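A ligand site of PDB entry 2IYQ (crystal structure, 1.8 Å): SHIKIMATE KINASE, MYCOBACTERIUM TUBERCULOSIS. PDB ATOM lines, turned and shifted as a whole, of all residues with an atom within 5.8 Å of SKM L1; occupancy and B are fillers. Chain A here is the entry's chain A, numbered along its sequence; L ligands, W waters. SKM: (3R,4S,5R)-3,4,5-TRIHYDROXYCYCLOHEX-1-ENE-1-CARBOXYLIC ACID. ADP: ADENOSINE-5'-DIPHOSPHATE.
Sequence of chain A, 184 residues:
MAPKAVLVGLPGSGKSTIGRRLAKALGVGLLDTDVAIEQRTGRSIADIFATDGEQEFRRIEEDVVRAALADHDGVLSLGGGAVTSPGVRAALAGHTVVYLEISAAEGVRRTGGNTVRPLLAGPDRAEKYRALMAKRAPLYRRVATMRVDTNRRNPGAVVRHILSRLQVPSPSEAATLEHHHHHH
N of Lys 15 lies within hydrogen-bond range of O3B of ADP L2 (2.9 Å). The side-chain amino group (NZ) of Lys 15 lies within salt-bridge range of an oxygen (O3B) of ADP L2 (2.9 Å). O2 of SKM L1 is in salt-bridge range of NH1 of Arg 136 (2.7 Å). An oxygen (O2B) of ADP L2 lies within salt-bridge range of the guanidinium group (NH2) of Arg 117 (2.9 Å). The backbone NH (N) of Gly 81 sits close to an oxygen (O3) of SKM L1, at 3.4 Å. An oxygen (O12) of SKM L1 sits at hydrogen-bond distance from the side-chain carboxylate (OD1) of Asp 34 (2.6 Å). The guanidinium group (NH2) of Arg 58 lies within salt-bridge range of an oxygen (O3) of SKM L1 (2.7 Å). An oxygen (O11) of SKM L1 is in hydrogen-bond range of the backbone NH (N) of Gly 80, 3.0 Å away.
The guanidinium group of Arg 58 sits close to the backbone carbonyl oxygen of Gly 81, 3.1 Å away. The guanidinium group of Arg 136 lies within hydrogen-bond range of the backbone carbonyl oxygen of Gly 80. The guanidinium group (NH1) of Arg 58 lies within salt-bridge range of the side-chain carboxylate (OE1) of Glu 61, at 3.0 Å. The side-chain carboxylate of Glu 54 is in salt-bridge range of the guanidinium group of Arg 58, 3.2 Å away. The backbone carbonyl oxygen of Gly 80 sits at hydrogen-bond distance from the side-chain hydroxyl of Tyr 140.
Merely in contact with SKM L1: Pro 11, Ile 45, Phe 57, Gly 79, Pro 118 and Leu 119. Hydrophobic or aromatic side chains within 4 Å of SKM L1: Pro 11, Ile 45, Phe 57, Pro 118 and Leu 119. 11 residues have an atom within 4 Å of SKM L1: Pro 11, Asp 34, Ile 45, Phe 57, Arg 58, Gly 79, Gly 80, Gly 81, Pro 118, Leu 119 and Arg 136.
Water W2 bridges an oxygen (O7) of SKM L1 (2.6 Å) and the backbone carbonyl oxygen (O) of Val 116 (2.8 Å). Water W4 lies within hydrogen-bond range of O11 of SKM L1 (2.7 Å), NZ of Lys 15 (2.9 Å) and O2B of ADP L2 (3.0 Å). Water W1 lies within hydrogen-bond range of the backbone NH of Leu 119 (2.9 Å) and an oxygen (O7) of SKM L1 (2.9 Å).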
ATOM      1  N   PRO A  11      16.278  -4.649  14.697  1.00  0.00           N
ATOM      2  CA  PRO A  11      16.523  -6.009  14.200  1.00  0.00           C
ATOM      3  C   PRO A  11      15.327  -6.904  14.389  1.00  0.00           C
ATOM      4  O   PRO A  11      14.704  -6.852  15.425  1.00  0.00           O
ATOM      5  CB  PRO A  11      17.675  -6.514  15.077  1.00  0.00           C
ATOM      6  CG  PRO A  11      17.848  -5.497  16.149  1.00  0.00           C
ATOM      7  CD  PRO A  11      17.348  -4.218  15.634  1.00  0.00           C
ATOM      8  N   LYS A  15      12.731  -5.580   8.100  1.00  0.00           N
ATOM      9  CA  LYS A  15      13.244  -4.722   6.972  1.00  0.00           C
ATOM     10  C   LYS A  15      13.624  -5.506   5.713  1.00  0.00           C
ATOM     11  O   LYS A  15      13.288  -5.102   4.577  1.00  0.00           O
ATOM     12  CB  LYS A  15      14.443  -3.873   7.429  1.00  0.00           C
ATOM     13  CG  LYS A  15      14.025  -2.991   8.603  1.00  0.00           C
ATOM     14  CD  LYS A  15      15.248  -2.147   9.089  1.00  0.00           C
ATOM     15  CE  LYS A  15      16.336  -3.007   9.702  1.00  0.00           C
ATOM     16  NZ  LYS A  15      15.971  -3.728  10.938  1.00  0.00           N
ATOM     17  N   ASP A  34      22.814  -3.642   4.598  1.00  0.00           N
ATOM     18  CA  ASP A  34      23.685  -4.634   5.221  1.00  0.00           C
ATOM     19  C   ASP A  34      24.368  -5.470   4.148  1.00  0.00           C
ATOM     20  O   ASP A  34      25.574  -5.714   4.214  1.00  0.00           O
ATOM     21  CB  ASP A  34      22.894  -5.569   6.159  1.00  0.00           C
ATOM     22  CG  ASP A  34      22.510  -4.924   7.490  1.00  0.00           C
ATOM     23  OD1 ASP A  34      23.034  -3.831   7.849  1.00  0.00           O
ATOM     24  OD2 ASP A  34      21.688  -5.552   8.181  1.00  0.00           O
ATOM     25  N   ILE A  45      29.337  -8.780   8.348  1.00  0.00           N
ATOM     26  CA  ILE A  45      29.094  -7.708   9.323  1.00  0.00           C
ATOM     27  C   ILE A  45      29.704  -8.041  10.680  1.00  0.00           C
ATOM     28  O   ILE A  45      30.270  -7.168  11.355  1.00  0.00           O
ATOM     29  CB  ILE A  45      27.569  -7.439   9.497  1.00  0.00           C
ATOM     30  CG1 ILE A  45      27.014  -6.864   8.184  1.00  0.00           C
ATOM     31  CG2 ILE A  45      27.306  -6.535  10.741  1.00  0.00           C
ATOM     32  CD1 ILE A  45      25.576  -6.407   8.276  1.00  0.00           C
ATOM     33  N   PHE A  49      32.605  -5.783  12.722  1.00  0.00           N
ATOM     34  CA  PHE A  49      32.391  -5.443  14.113  1.00  0.00           C
ATOM     35  C   PHE A  49      33.529  -6.004  14.979  1.00  0.00           C
ATOM     36  O   PHE A  49      34.041  -5.320  15.863  1.00  0.00           O
ATOM     37  CB  PHE A  49      31.058  -5.989  14.607  1.00  0.00           C
ATOM     38  CG  PHE A  49      29.917  -5.027  14.513  1.00  0.00           C
ATOM     39  CD1 PHE A  49      29.266  -4.801  13.301  1.00  0.00           C
ATOM     40  CD2 PHE A  49      29.471  -4.383  15.632  1.00  0.00           C
ATOM     41  CE1 PHE A  49      28.180  -3.910  13.248  1.00  0.00           C
ATOM     42  CE2 PHE A  49      28.393  -3.476  15.596  1.00  0.00           C
ATOM     43  CZ  PHE A  49      27.751  -3.252  14.404  1.00  0.00           C
ATOM     44  N   GLU A  54      32.256  -1.266  15.967  1.00  0.00           N
ATOM     45  CA  GLU A  54      31.044  -0.583  15.575  1.00  0.00           C
ATOM     46  C   GLU A  54      31.256   0.786  14.937  1.00  0.00           C
ATOM     47  O   GLU A  54      30.611   1.080  13.960  1.00  0.00           O
ATOM     48  CB  GLU A  54      30.101  -0.469  16.781  1.00  0.00           C
ATOM     49  CG  GLU A  54      28.841   0.345  16.517  1.00  0.00           C
ATOM     50  CD  GLU A  54      27.734   0.085  17.525  1.00  0.00           C
ATOM     51  OE1 GLU A  54      27.910  -0.752  18.438  1.00  0.00           O
ATOM     52  OE2 GLU A  54      26.674   0.734  17.387  1.00  0.00           O
ATOM     53  N   PHE A  57      32.242   0.365  11.345  1.00  0.00           N
ATOM     54  CA  PHE A  57      31.014  -0.108  10.691  1.00  0.00           C
ATOM     55  C   PHE A  57      30.050   1.037  10.417  1.00  0.00           C
ATOM     56  O   PHE A  57      29.535   1.140   9.323  1.00  0.00           O
ATOM     57  CB  PHE A  57      30.293  -1.184  11.507  1.00  0.00           C
ATOM     58  CG  PHE A  57      29.044  -1.660  10.843  1.00  0.00           C
ATOM     59  CD1 PHE A  57      29.107  -2.581   9.809  1.00  0.00           C
ATOM     60  CD2 PHE A  57      27.813  -1.119  11.201  1.00  0.00           C
ATOM     61  CE1 PHE A  57      27.965  -3.017   9.173  1.00  0.00           C
ATOM     62  CE2 PHE A  57      26.634  -1.555  10.547  1.00  0.00           C
ATOM     63  CZ  PHE A  57      26.736  -2.523   9.533  1.00  0.00           C
ATOM     64  N   ARG A  58      29.828   1.904  11.400  1.00  0.00           N
ATOM     65  CA  ARG A  58      28.903   3.033  11.235  1.00  0.00           C
ATOM     66  C   ARG A  58      29.369   4.052  10.181  1.00  0.00           C
ATOM     67  O   ARG A  58      28.548   4.621   9.449  1.00  0.00           O
ATOM     68  CB  ARG A  58      28.638   3.743  12.571  1.00  0.00           C
ATOM     69  CG  ARG A  58      28.036   2.863  13.645  1.00  0.00           C
ATOM     70  CD  ARG A  58      26.598   2.414  13.339  1.00  0.00           C
ATOM     71  NE  ARG A  58      26.132   1.419  14.317  1.00  0.00           N
ATOM     72  CZ  ARG A  58      25.169   0.522  14.109  1.00  0.00           C
ATOM     73  NH1 ARG A  58      24.518   0.515  12.972  1.00  0.00           N
ATOM     74  NH2 ARG A  58      24.823  -0.334  15.046  1.00  0.00           N
ATOM     75  N   GLU A  61      28.787   2.313   6.865  1.00  0.00           N
ATOM     76  CA  GLU A  61      27.347   2.281   6.716  1.00  0.00           C
ATOM     77  C   GLU A  61      26.802   3.658   6.280  1.00  0.00           C
ATOM     78  O   GLU A  61      26.017   3.717   5.337  1.00  0.00           O
ATOM     79  CB  GLU A  61      26.741   1.807   8.029  1.00  0.00           C
ATOM     80  CG  GLU A  61      25.173   1.772   8.034  1.00  0.00           C
ATOM     81  CD  GLU A  61      24.611   1.377   9.376  1.00  0.00           C
ATOM     82  OE1 GLU A  61      25.024   2.000  10.408  1.00  0.00           O
ATOM     83  OE2 GLU A  61      23.766   0.447   9.350  1.00  0.00           O
ATOM     84  N   LEU A  78      17.371  -0.151   5.473  1.00  0.00           N
ATOM     85  CA  LEU A  78      18.585   0.233   6.266  1.00  0.00           C
ATOM     86  C   LEU A  78      18.932  -0.809   7.347  1.00  0.00           C
ATOM     87  O   LEU A  78      18.069  -1.556   7.794  1.00  0.00           O
ATOM     88  CB  LEU A  78      18.391   1.576   6.925  1.00  0.00           C
ATOM     89  CG  LEU A  78      18.104   2.747   5.991  1.00  0.00           C
ATOM     90  CD1 LEU A  78      18.300   4.053   6.781  1.00  0.00           C
ATOM     91  CD2 LEU A  78      18.944   2.719   4.767  1.00  0.00           C
ATOM     92  N   GLY A  79      20.205  -0.895   7.724  1.00  0.00           N
ATOM     93  CA  GLY A  79      20.541  -1.703   8.907  1.00  0.00           C
ATOM     94  C   GLY A  79      19.802  -1.198  10.127  1.00  0.00           C
ATOM     95  O   GLY A  79      19.420  -0.017  10.235  1.00  0.00           O
ATOM     96  N   GLY A  80      19.611  -2.084  11.112  1.00  0.00           N
ATOM     97  CA  GLY A  80      18.789  -1.702  12.245  1.00  0.00           C
ATOM     98  C   GLY A  80      19.333  -0.543  13.078  1.00  0.00           C
ATOM     99  O   GLY A  80      18.575   0.158  13.750  1.00  0.00           O
ATOM    100  N   GLY A  81      20.646  -0.357  13.032  1.00  0.00           N
ATOM    101  CA  GLY A  81      21.275   0.706  13.837  1.00  0.00           C
ATOM    102  C   GLY A  81      21.734   1.915  13.061  1.00  0.00           C
ATOM    103  O   GLY A  81      22.427   2.777  13.576  1.00  0.00           O
ATOM    104  N   ALA A  82      21.324   2.001  11.807  1.00  0.00           N
ATOM    105  CA  ALA A  82      21.759   3.132  10.978  1.00  0.00           C
ATOM    106  C   ALA A  82      21.291   4.461  11.518  1.00  0.00           C
ATOM    107  O   ALA A  82      22.006   5.450  11.375  1.00  0.00           O
ATOM    108  CB  ALA A  82      21.313   2.959   9.486  1.00  0.00           C
ATOM    109  N   VAL A 116      23.858 -13.861  13.450  1.00  0.00           N
ATOM    110  CA  VAL A 116      24.642 -12.967  12.572  1.00  0.00           C
ATOM    111  C   VAL A 116      24.569 -11.474  12.966  1.00  0.00           C
ATOM    112  O   VAL A 116      25.164 -10.628  12.261  1.00  0.00           O
ATOM    113  CB  VAL A 116      24.218 -13.150  11.084  1.00  0.00           C
ATOM    114  CG1 VAL A 116      24.654 -14.515  10.576  1.00  0.00           C
ATOM    115  CG2 VAL A 116      22.718 -12.970  10.890  1.00  0.00           C
ATOM    116  N   ARG A 117      23.913 -11.179  14.099  1.00  0.00           N
ATOM    117  CA  ARG A 117      23.803  -9.821  14.669  1.00  0.00           C
ATOM    118  C   ARG A 117      24.657  -9.631  15.962  1.00  0.00           C
ATOM    119  O   ARG A 117      24.228 -10.030  17.059  1.00  0.00           O
ATOM    120  CB  ARG A 117      22.328  -9.487  14.942  1.00  0.00           C
ATOM    121  CG  ARG A 117      21.450  -9.492  13.665  1.00  0.00           C
ATOM    122  CD  ARG A 117      20.087  -8.854  13.926  1.00  0.00           C
ATOM    123  NE  ARG A 117      19.012  -9.078  12.915  1.00  0.00           N
ATOM    124  CZ  ARG A 117      18.207 -10.150  12.824  1.00  0.00           C
ATOM    125  NH1 ARG A 117      18.366 -11.218  13.629  1.00  0.00           N
ATOM    126  NH2 ARG A 117      17.247 -10.175  11.885  1.00  0.00           N
ATOM    127  N   PRO A 118      25.842  -8.997  15.827  1.00  0.00           N
ATOM    128  CA  PRO A 118      26.767  -8.659  16.935  1.00  0.00           C
ATOM    129  C   PRO A 118      26.133  -8.030  18.165  1.00  0.00           C
ATOM    130  O   PRO A 118      26.550  -8.282  19.304  1.00  0.00           O
ATOM    131  CB  PRO A 118      27.726  -7.654  16.293  1.00  0.00           C
ATOM    132  CG  PRO A 118      27.792  -8.056  14.891  1.00  0.00           C
ATOM    133  CD  PRO A 118      26.416  -8.598  14.529  1.00  0.00           C
ATOM    134  N   LEU A 119      25.133  -7.180  17.954  1.00  0.00           N
ATOM    135  CA  LEU A 119      24.579  -6.439  19.082  1.00  0.00           C
ATOM    136  C   LEU A 119      23.510  -7.226  19.829  1.00  0.00           C
ATOM    137  O   LEU A 119      23.065  -6.806  20.895  1.00  0.00           O
ATOM    138  CB  LEU A 119      24.104  -5.043  18.636  1.00  0.00           C
ATOM    139  CG  LEU A 119      25.236  -4.169  18.062  1.00  0.00           C
ATOM    140  CD1 LEU A 119      24.700  -2.806  17.641  1.00  0.00           C
ATOM    141  CD2 LEU A 119      26.403  -3.992  19.055  1.00  0.00           C
ATOM    142  N   LEU A 132      17.985  -1.955  23.384  1.00  0.00           N
ATOM    143  CA  LEU A 132      18.057  -1.375  22.019  1.00  0.00           C
ATOM    144  C   LEU A 132      16.768  -0.627  21.729  1.00  0.00           C
ATOM    145  O   LEU A 132      16.746   0.480  21.189  1.00  0.00           O
ATOM    146  CB  LEU A 132      18.280  -2.466  20.983  1.00  0.00           C
ATOM    147  CG  LEU A 132      19.546  -2.569  20.120  1.00  0.00           C
ATOM    148  CD1 LEU A 132      20.780  -2.137  20.833  1.00  0.00           C
ATOM    149  CD2 LEU A 132      19.674  -3.972  19.584  1.00  0.00           C
ATOM    150  N   ARG A 136      16.703   3.293  20.812  1.00  0.00           N
ATOM    151  CA  ARG A 136      16.393   3.665  19.408  1.00  0.00           C
ATOM    152  C   ARG A 136      14.995   4.114  19.012  1.00  0.00           C
ATOM    153  O   ARG A 136      14.835   4.771  17.998  1.00  0.00           O
ATOM    154  CB  ARG A 136      16.837   2.562  18.519  1.00  0.00           C
ATOM    155  CG  ARG A 136      18.268   2.144  18.749  1.00  0.00           C
ATOM    156  CD  ARG A 136      18.580   1.023  17.889  1.00  0.00           C
ATOM    157  NE  ARG A 136      19.972   0.694  17.877  1.00  0.00           N
ATOM    158  CZ  ARG A 136      20.464  -0.340  17.221  1.00  0.00           C
ATOM    159  NH1 ARG A 136      19.705  -1.071  16.418  1.00  0.00           N
ATOM    160  NH2 ARG A 136      21.745  -0.602  17.326  1.00  0.00           N
ATOM    161  N   TYR A 140      14.002   6.195  15.602  1.00  0.00           N
ATOM    162  CA  TYR A 140      13.104   5.772  14.531  1.00  0.00           C
ATOM    163  C   TYR A 140      11.907   6.698  14.362  1.00  0.00           C
ATOM    164  O   TYR A 140      11.524   7.044  13.238  1.00  0.00           O
ATOM    165  CB  TYR A 140      12.616   4.347  14.769  1.00  0.00           C
ATOM    166  CG  TYR A 140      13.691   3.307  14.814  1.00  0.00           C
ATOM    167  CD1 TYR A 140      14.553   3.103  13.786  1.00  0.00           C
ATOM    168  CD2 TYR A 140      13.749   2.423  15.894  1.00  0.00           C
ATOM    169  CE1 TYR A 140      15.518   2.090  13.876  1.00  0.00           C
ATOM    170  CE2 TYR A 140      14.665   1.442  16.003  1.00  0.00           C
ATOM    171  CZ  TYR A 140      15.539   1.242  15.019  1.00  0.00           C
ATOM    172  OH  TYR A 140      16.494   0.231  15.089  1.00  0.00           O
HETATM  173  O12 SKM L   1      23.289  -3.570  10.457  1.00  0.00           O
HETATM  174  C8  SKM L   1      23.176  -4.871  11.027  1.00  0.00           C
HETATM  175  C6  SKM L   1      24.199  -4.944  12.157  1.00  0.00           C
HETATM  176  O7  SKM L   1      24.251  -6.260  12.737  1.00  0.00           O
HETATM  177  C5  SKM L   1      23.878  -3.889  13.209  1.00  0.00           C
HETATM  178  C4  SKM L   1      22.429  -3.816  13.609  1.00  0.00           C
HETATM  179  C1  SKM L   1      22.028  -2.998  14.732  1.00  0.00           C
HETATM  180  O2  SKM L   1      20.921  -3.154  15.315  1.00  0.00           O
HETATM  181  O3  SKM L   1      22.786  -2.051  15.047  1.00  0.00           O
HETATM  182  C10 SKM L   1      21.474  -4.432  12.865  1.00  0.00           C
HETATM  183  C9  SKM L   1      21.765  -5.159  11.585  1.00  0.00           C
HETATM  184  O11 SKM L   1      20.758  -4.770  10.632  1.00  0.00           O
HETATM  185  PB  ADP L   2      15.240  -7.215   9.818  1.00  0.00           P
HETATM  186  O1B ADP L   2      15.791  -7.108   8.431  1.00  0.00           O
HETATM  187  O2B ADP L   2      16.340  -7.642  10.768  1.00  0.00           O
HETATM  188  O3B ADP L   2      14.403  -6.052  10.380  1.00  0.00           O
HETATM  189  PA  ADP L   2      14.125  -9.719   8.820  1.00  0.00           P
HETATM  190  O1A ADP L   2      15.441 -10.364   8.506  1.00  0.00           O
HETATM  191  O2A ADP L   2      13.357  -9.321   7.605  1.00  0.00           O
HETATM  192  O3A ADP L   2      14.195  -8.474   9.847  1.00  0.00           O
HETATM  193  O5' ADP L   2      13.002 -10.636   9.549  1.00  0.00           O
HETATM  194  C5' ADP L   2      13.391 -11.405  10.709  1.00  0.00           C
HETATM  195  C4' ADP L   2      12.549 -12.695  10.769  1.00  0.00           C
HETATM  196  O4' ADP L   2      11.266 -12.262  11.076  1.00  0.00           O
HETATM  197  C3' ADP L   2      12.497 -13.463   9.452  1.00  0.00           C
HETATM  198  O3' ADP L   2      12.396 -14.920   9.572  1.00  0.00           O
HETATM  199  C2' ADP L   2      11.218 -13.054   8.875  1.00  0.00           C
HETATM  200  O2' ADP L   2      10.631 -14.158   8.201  1.00  0.00           O
HETATM  201  C1' ADP L   2      10.379 -12.716  10.111  1.00  0.00           C
HETATM  202  N9  ADP L   2       9.357 -11.719   9.933  1.00  0.00           N
HETATM  203  C8  ADP L   2       9.561 -10.450   9.492  1.00  0.00           C
HETATM  204  N7  ADP L   2       8.390  -9.832   9.451  1.00  0.00           N
HETATM  205  C5  ADP L   2       7.424 -10.653   9.911  1.00  0.00           C
HETATM  206  C6  ADP L   2       6.008 -10.528  10.078  1.00  0.00           C
HETATM  207  N6  ADP L   2       5.345  -9.412   9.826  1.00  0.00           N
HETATM  208  N1  ADP L   2       5.285 -11.629  10.556  1.00  0.00           N
HETATM  209  C2  ADP L   2       6.013 -12.757  10.818  1.00  0.00           C
HETATM  210  N3  ADP L   2       7.319 -12.940  10.681  1.00  0.00           N
HETATM  211  C4  ADP L   2       8.059 -11.889  10.212  1.00  0.00           C
HETATM  212  O   HOH W   1      23.624  -6.384  15.610  1.00  0.00           O
HETATM  213  O   HOH W   2      24.058  -8.346  11.144  1.00  0.00           O
HETATM  214  O   HOH W   3      22.859  -1.179  11.392  1.00  0.00           O
HETATM  215  O   HOH W   4      18.263  -5.437  11.358  1.00  0.00           O
HETATM  216  O   HOH W   5      21.192  -5.822  16.353  1.00  0.00           O
